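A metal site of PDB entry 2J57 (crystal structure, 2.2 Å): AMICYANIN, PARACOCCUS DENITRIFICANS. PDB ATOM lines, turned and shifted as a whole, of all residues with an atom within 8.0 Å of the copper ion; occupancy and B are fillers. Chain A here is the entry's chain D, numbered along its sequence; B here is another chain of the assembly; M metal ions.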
ATOM      1  N   ILE A  25     -21.566 -33.550 -19.013  1.00  0.00           N
ATOM      2  CA  ILE A  25     -21.207 -32.320 -18.308  1.00  0.00           C
ATOM      3  C   ILE A  25     -19.713 -32.222 -18.312  1.00  0.00           C
ATOM      4  O   ILE A  25     -19.037 -33.155 -17.874  1.00  0.00           O
ATOM      5  CB  ILE A  25     -21.721 -32.315 -16.851  1.00  0.00           C
ATOM      6  CG1 ILE A  25     -23.250 -32.536 -16.827  1.00  0.00           C
ATOM      7  CG2 ILE A  25     -21.242 -31.065 -16.103  1.00  0.00           C
ATOM      8  CD1 ILE A  25     -23.799 -33.035 -15.527  1.00  0.00           C
ATOM      9  N   MET A  28     -17.599 -26.921 -17.274  1.00  0.00           N
ATOM     10  CA  MET A  28     -18.595 -26.117 -16.513  1.00  0.00           C
ATOM     11  C   MET A  28     -19.852 -25.845 -17.297  1.00  0.00           C
ATOM     12  O   MET A  28     -20.416 -24.758 -17.129  1.00  0.00           O
ATOM     13  CB  MET A  28     -18.051 -24.734 -16.011  1.00  0.00           C
ATOM     14  CG  MET A  28     -16.764 -24.781 -15.262  1.00  0.00           C
ATOM     15  SD  MET A  28     -16.991 -25.738 -13.788  1.00  0.00           S
ATOM     16  CE  MET A  28     -18.262 -24.745 -12.919  1.00  0.00           C
ATOM     17  N   LYS A  29     -20.283 -26.824 -18.117  1.00  0.00           N
ATOM     18  CA  LYS A  29     -21.583 -26.732 -18.745  1.00  0.00           C
ATOM     19  C   LYS A  29     -22.266 -28.029 -19.213  1.00  0.00           C
ATOM     20  O   LYS A  29     -21.637 -29.069 -19.408  1.00  0.00           O
ATOM     21  CB  LYS A  29     -21.602 -25.682 -19.851  1.00  0.00           C
ATOM     22  CG  LYS A  29     -20.602 -25.839 -20.961  1.00  0.00           C
ATOM     23  CD  LYS A  29     -20.511 -24.479 -21.672  1.00  0.00           C
ATOM     24  CE  LYS A  29     -19.143 -24.246 -22.272  1.00  0.00           C
ATOM     25  NZ  LYS A  29     -18.955 -25.229 -23.407  1.00  0.00           N
ATOM     26  N   TYR A  30     -23.585 -27.921 -19.371  1.00  0.00           N
ATOM     27  CA  TYR A  30     -24.382 -29.012 -19.870  1.00  0.00           C
ATOM     28  C   TYR A  30     -24.186 -29.025 -21.383  1.00  0.00           C
ATOM     29  O   TYR A  30     -24.556 -28.075 -22.072  1.00  0.00           O
ATOM     30  CB  TYR A  30     -25.836 -28.794 -19.530  1.00  0.00           C
ATOM     31  CG  TYR A  30     -26.164 -28.745 -18.045  1.00  0.00           C
ATOM     32  CD1 TYR A  30     -25.997 -29.875 -17.233  1.00  0.00           C
ATOM     33  CD2 TYR A  30     -26.725 -27.565 -17.460  1.00  0.00           C
ATOM     34  CE1 TYR A  30     -26.330 -29.843 -15.865  1.00  0.00           C
ATOM     35  CE2 TYR A  30     -27.091 -27.508 -16.061  1.00  0.00           C
ATOM     36  CZ  TYR A  30     -26.875 -28.655 -15.293  1.00  0.00           C
ATOM     37  OH  TYR A  30     -27.217 -28.696 -13.977  1.00  0.00           O
ATOM     38  N   ASN A  47     -21.330 -36.739 -15.402  1.00  0.00           N
ATOM     39  CA  ASN A  47     -20.280 -35.741 -15.132  1.00  0.00           C
ATOM     40  C   ASN A  47     -18.945 -36.200 -15.641  1.00  0.00           C
ATOM     41  O   ASN A  47     -18.414 -37.231 -15.177  1.00  0.00           O
ATOM     42  CB  ASN A  47     -20.101 -35.519 -13.636  1.00  0.00           C
ATOM     43  CG  ASN A  47     -19.191 -34.336 -13.321  1.00  0.00           C
ATOM     44  OD1 ASN A  47     -18.733 -33.610 -14.219  1.00  0.00           O
ATOM     45  ND2 ASN A  47     -18.957 -34.113 -12.032  1.00  0.00           N
ATOM     46  N   GLU A  49     -16.039 -34.267 -15.567  1.00  0.00           N
ATOM     47  CA  GLU A  49     -14.933 -33.614 -14.896  1.00  0.00           C
ATOM     48  C   GLU A  49     -14.961 -33.768 -13.383  1.00  0.00           C
ATOM     49  O   GLU A  49     -15.911 -34.253 -12.796  1.00  0.00           O
ATOM     50  CB  GLU A  49     -14.910 -32.162 -15.262  1.00  0.00           C
ATOM     51  CG  GLU A  49     -16.227 -31.452 -14.907  1.00  0.00           C
ATOM     52  CD  GLU A  49     -16.156 -30.002 -15.315  1.00  0.00           C
ATOM     53  OE1 GLU A  49     -14.974 -29.518 -15.414  1.00  0.00           O
ATOM     54  OE2 GLU A  49     -17.231 -29.370 -15.537  1.00  0.00           O
ATOM     55  N   MET A  51     -14.732 -31.303 -10.923  1.00  0.00           N
ATOM     56  CA  MET A  51     -15.737 -30.342 -10.382  1.00  0.00           C
ATOM     57  C   MET A  51     -17.099 -30.999 -10.220  1.00  0.00           C
ATOM     58  O   MET A  51     -17.689 -31.415 -11.228  1.00  0.00           O
ATOM     59  CB  MET A  51     -15.909 -29.139 -11.342  1.00  0.00           C
ATOM     60  CG  MET A  51     -16.956 -28.098 -10.904  1.00  0.00           C
ATOM     61  SD  MET A  51     -16.462 -27.357  -9.334  1.00  0.00           S
ATOM     62  CE  MET A  51     -15.149 -26.336 -10.007  1.00  0.00           C
ATOM     63  N   PRO A  52     -17.588 -31.158  -8.970  1.00  0.00           N
ATOM     64  CA  PRO A  52     -18.964 -31.711  -8.854  1.00  0.00           C
ATOM     65  C   PRO A  52     -20.049 -30.857  -9.527  1.00  0.00           C
ATOM     66  O   PRO A  52     -19.896 -29.647  -9.654  1.00  0.00           O
ATOM     67  CB  PRO A  52     -19.177 -31.849  -7.326  1.00  0.00           C
ATOM     68  CG  PRO A  52     -17.769 -31.966  -6.781  1.00  0.00           C
ATOM     69  CD  PRO A  52     -16.955 -31.007  -7.650  1.00  0.00           C
ATOM     70  N   HIS A  53     -21.121 -31.525  -9.977  1.00  0.00           N
ATOM     71  CA  HIS A  53     -22.285 -30.914 -10.641  1.00  0.00           C
ATOM     72  C   HIS A  53     -23.519 -31.739 -10.352  1.00  0.00           C
ATOM     73  O   HIS A  53     -23.412 -32.903  -9.995  1.00  0.00           O
ATOM     74  CB  HIS A  53     -22.127 -30.780 -12.148  1.00  0.00           C
ATOM     75  CG  HIS A  53     -20.827 -30.193 -12.608  1.00  0.00           C
ATOM     76  ND1 HIS A  53     -20.566 -28.838 -12.591  1.00  0.00           N
ATOM     77  CD2 HIS A  53     -19.736 -30.774 -13.166  1.00  0.00           C
ATOM     78  CE1 HIS A  53     -19.371 -28.609 -13.120  1.00  0.00           C
ATOM     79  NE2 HIS A  53     -18.852 -29.771 -13.469  1.00  0.00           N
ATOM     80  N   ASN A  54     -24.699 -31.113 -10.469  1.00  0.00           N
ATOM     81  CA  ASN A  54     -25.974 -31.818 -10.386  1.00  0.00           C
ATOM     82  C   ASN A  54     -26.998 -31.251 -11.362  1.00  0.00           C
ATOM     83  O   ASN A  54     -26.631 -30.445 -12.225  1.00  0.00           O
ATOM     84  CB  ASN A  54     -26.480 -31.837  -8.965  1.00  0.00           C
ATOM     85  CG  ASN A  54     -27.139 -30.506  -8.495  1.00  0.00           C
ATOM     86  OD1 ASN A  54     -26.982 -29.391  -9.085  1.00  0.00           O
ATOM     87  ND2 ASN A  54     -27.863 -30.627  -7.383  1.00  0.00           N
ATOM     88  N   VAL A  55     -28.254 -31.745 -11.252  1.00  0.00           N
ATOM     89  CA  VAL A  55     -29.395 -31.112 -11.920  1.00  0.00           C
ATOM     90  C   VAL A  55     -30.406 -30.745 -10.851  1.00  0.00           C
ATOM     91  O   VAL A  55     -30.553 -31.475  -9.853  1.00  0.00           O
ATOM     92  CB  VAL A  55     -30.068 -32.002 -13.042  1.00  0.00           C
ATOM     93  CG1 VAL A  55     -29.044 -32.323 -14.079  1.00  0.00           C
ATOM     94  CG2 VAL A  55     -30.612 -33.279 -12.487  1.00  0.00           C
ATOM     95  N   MET A  71     -25.067 -34.540  -6.046  1.00  0.00           N
ATOM     96  CA  MET A  71     -23.869 -34.064  -6.758  1.00  0.00           C
ATOM     97  C   MET A  71     -23.143 -35.230  -7.379  1.00  0.00           C
ATOM     98  O   MET A  71     -22.830 -36.217  -6.683  1.00  0.00           O
ATOM     99  CB  MET A  71     -22.877 -33.349  -5.809  1.00  0.00           C
ATOM    100  CG  MET A  71     -23.450 -32.079  -5.140  1.00  0.00           C
ATOM    101  SD  MET A  71     -24.085 -30.824  -6.305  1.00  0.00           S
ATOM    102  CE  MET A  71     -22.623 -30.300  -7.162  1.00  0.00           C
ATOM    103  N   MET A  72     -22.888 -35.129  -8.668  1.00  0.00           N
ATOM    104  CA  MET A  72     -22.068 -36.118  -9.330  1.00  0.00           C
ATOM    105  C   MET A  72     -20.561 -35.754  -9.230  1.00  0.00           C
ATOM    106  O   MET A  72     -20.126 -34.705  -9.735  1.00  0.00           O
ATOM    107  CB  MET A  72     -22.465 -36.264 -10.789  1.00  0.00           C
ATOM    108  CG  MET A  72     -23.844 -36.949 -10.987  1.00  0.00           C
ATOM    109  SD  MET A  72     -24.485 -36.639 -12.648  1.00  0.00           S
ATOM    110  CE  MET A  72     -25.222 -34.996 -12.470  1.00  0.00           C
ATOM    111  N   HIS A  91     -30.942 -26.406 -13.457  1.00  0.00           N
ATOM    112  CA  HIS A  91     -29.702 -25.656 -13.292  1.00  0.00           C
ATOM    113  C   HIS A  91     -28.816 -26.461 -12.376  1.00  0.00           C
ATOM    114  O   HIS A  91     -29.282 -27.368 -11.739  1.00  0.00           O
ATOM    115  CB  HIS A  91     -29.983 -24.247 -12.733  1.00  0.00           C
ATOM    116  CG  HIS A  91     -30.264 -24.204 -11.249  1.00  0.00           C
ATOM    117  ND1 HIS A  91     -31.524 -24.372 -10.711  1.00  0.00           N
ATOM    118  CD2 HIS A  91     -29.430 -24.022 -10.193  1.00  0.00           C
ATOM    119  CE1 HIS A  91     -31.469 -24.304  -9.399  1.00  0.00           C
ATOM    120  NE2 HIS A  91     -30.212 -24.091  -9.054  1.00  0.00           N
ATOM    121  N   CYS A  92     -27.530 -26.128 -12.298  1.00  0.00           N
ATOM    122  CA  CYS A  92     -26.654 -26.756 -11.306  1.00  0.00           C
ATOM    123  C   CYS A  92     -26.757 -25.944 -10.008  1.00  0.00           C
ATOM    124  O   CYS A  92     -26.625 -24.709 -10.035  1.00  0.00           O
ATOM    125  CB  CYS A  92     -25.206 -26.772 -11.823  1.00  0.00           C
ATOM    126  SG  CYS A  92     -24.091 -27.766 -10.817  1.00  0.00           S
ATOM    127  N   THR A  93     -27.028 -26.638  -8.899  1.00  0.00           N
ATOM    128  CA  THR A  93     -27.151 -26.050  -7.575  1.00  0.00           C
ATOM    129  C   THR A  93     -26.036 -25.042  -7.175  1.00  0.00           C
ATOM    130  O   THR A  93     -26.356 -23.893  -6.868  1.00  0.00           O
ATOM    131  CB  THR A  93     -27.286 -27.134  -6.510  1.00  0.00           C
ATOM    132  OG1 THR A  93     -28.403 -27.933  -6.865  1.00  0.00           O
ATOM    133  CG2 THR A  93     -27.512 -26.575  -5.126  1.00  0.00           C
ATOM    134  N   PRO A  94     -24.748 -25.471  -7.148  1.00  0.00           N
ATOM    135  CA  PRO A  94     -23.804 -24.417  -6.755  1.00  0.00           C
ATOM    136  C   PRO A  94     -23.418 -23.521  -7.933  1.00  0.00           C
ATOM    137  O   PRO A  94     -22.624 -22.611  -7.766  1.00  0.00           O
ATOM    138  CB  PRO A  94     -22.592 -25.223  -6.255  1.00  0.00           C
ATOM    139  CG  PRO A  94     -22.626 -26.540  -7.157  1.00  0.00           C
ATOM    140  CD  PRO A  94     -24.084 -26.772  -7.421  1.00  0.00           C
ATOM    141  N   HIS A  95     -23.937 -23.817  -9.127  1.00  0.00           N
ATOM    142  CA  HIS A  95     -23.503 -23.108 -10.349  1.00  0.00           C
ATOM    143  C   HIS A  95     -24.714 -22.740 -11.165  1.00  0.00           C
ATOM    144  O   HIS A  95     -25.051 -23.447 -12.125  1.00  0.00           O
ATOM    145  CB  HIS A  95     -22.512 -23.962 -11.188  1.00  0.00           C
ATOM    146  CG  HIS A  95     -21.399 -24.567 -10.374  1.00  0.00           C
ATOM    147  ND1 HIS A  95     -20.905 -25.834 -10.602  1.00  0.00           N
ATOM    148  CD2 HIS A  95     -20.671 -24.065  -9.346  1.00  0.00           C
ATOM    149  CE1 HIS A  95     -19.937 -26.091  -9.739  1.00  0.00           C
ATOM    150  NE2 HIS A  95     -19.795 -25.038  -8.953  1.00  0.00           N
ATOM    151  N   PRO A  96     -25.408 -21.622 -10.775  1.00  0.00           N
ATOM    152  CA  PRO A  96     -26.691 -21.276 -11.449  1.00  0.00           C
ATOM    153  C   PRO A  96     -26.497 -20.800 -12.881  1.00  0.00           C
ATOM    154  O   PRO A  96     -27.477 -20.759 -13.645  1.00  0.00           O
ATOM    155  CB  PRO A  96     -27.295 -20.171 -10.554  1.00  0.00           C
ATOM    156  CG  PRO A  96     -26.512 -20.345  -9.231  1.00  0.00           C
ATOM    157  CD  PRO A  96     -25.130 -20.652  -9.688  1.00  0.00           C
ATOM    158  N   PHE A  97     -25.259 -20.502 -13.243  1.00  0.00           N
ATOM    159  CA  PHE A  97     -24.917 -20.203 -14.645  1.00  0.00           C
ATOM    160  C   PHE A  97     -25.038 -21.400 -15.634  1.00  0.00           C
ATOM    161  O   PHE A  97     -25.139 -21.187 -16.844  1.00  0.00           O
ATOM    162  CB  PHE A  97     -23.524 -19.553 -14.729  1.00  0.00           C
ATOM    163  CG  PHE A  97     -22.423 -20.336 -14.050  1.00  0.00           C
ATOM    164  CD1 PHE A  97     -21.700 -21.302 -14.746  1.00  0.00           C
ATOM    165  CD2 PHE A  97     -22.133 -20.130 -12.719  1.00  0.00           C
ATOM    166  CE1 PHE A  97     -20.705 -22.012 -14.116  1.00  0.00           C
ATOM    167  CE2 PHE A  97     -21.131 -20.855 -12.083  1.00  0.00           C
ATOM    168  CZ  PHE A  97     -20.416 -21.784 -12.795  1.00  0.00           C
ATOM    169  N   MET A  98     -24.989 -22.624 -15.113  1.00  0.00           N
ATOM    170  CA  MET A  98     -25.096 -23.842 -15.890  1.00  0.00           C
ATOM    171  C   MET A  98     -26.596 -24.109 -15.894  1.00  0.00           C
ATOM    172  O   MET A  98     -27.221 -24.415 -14.831  1.00  0.00           O
ATOM    173  CB  MET A  98     -24.330 -25.032 -15.272  1.00  0.00           C
ATOM    174  CG  MET A  98     -22.786 -24.949 -15.056  1.00  0.00           C
ATOM    175  SD  MET A  98     -22.199 -26.314 -13.938  1.00  0.00           S
ATOM    176  CE  MET A  98     -22.829 -27.730 -14.980  1.00  0.00           C
ATOM    177  N   GLU B 101     -17.747 -21.211  -8.602  1.00  0.00           N
ATOM    178  CA  GLU B 101     -17.121 -22.568  -8.395  1.00  0.00           C
ATOM    179  C   GLU B 101     -16.023 -22.583  -7.372  1.00  0.00           C
ATOM    180  O   GLU B 101     -15.844 -23.600  -6.629  1.00  0.00           O
ATOM    181  CB  GLU B 101     -16.293 -23.048  -9.593  1.00  0.00           C
ATOM    182  CG  GLU B 101     -16.910 -22.917 -10.878  1.00  0.00           C
ATOM    183  CD  GLU B 101     -16.655 -21.579 -11.468  1.00  0.00           C
ATOM    184  OE1 GLU B 101     -15.722 -21.414 -12.267  1.00  0.00           O
ATOM    185  OE2 GLU B 101     -17.459 -20.712 -11.150  1.00  0.00           O
HETATM  186 CU    CU M   1     -22.090 -27.390 -11.784  1.00  0.00          CU
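The backbone carbonyl oxygen (O) of His 53 sits at hydrogen-bond distance from the backbone NH (N) of Met 72 (2.6 Å).
A ring nitrogen (NE2) of His 53 lies close to the backbone carbonyl oxygen (O) of Met 51, 3.0 Å away.
The side-chain hydroxyl of Tyr 30 sits at hydrogen-bond distance from the backbone NH of Cys 92, at 3.1 Å.
The backbone NH (N) of Asn 54 lies close to the side-chain sulfur (SG) of Cys 92 (3.4 Å).
The side-chain carboxylate (OE2) of Glu 49 sits at hydrogen-bond distance from a ring nitrogen (NE2) of His 53, at 2.7 Å.
The copper ion is bound by a ring nitrogen (ND1) of His 53, the side-chain sulfur (SG) of Cys 92, a ring nitrogen (ND1) of His 95 and the side-chain sulfur (SD) of Met 98.
The copper ion has four donor atoms within binding distance.
Pro 52 touches the copper ion.
Five residues have an atom within 4 Å of the copper ion: Pro 52, His 53, Cys 92, His 95 and Met 98.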
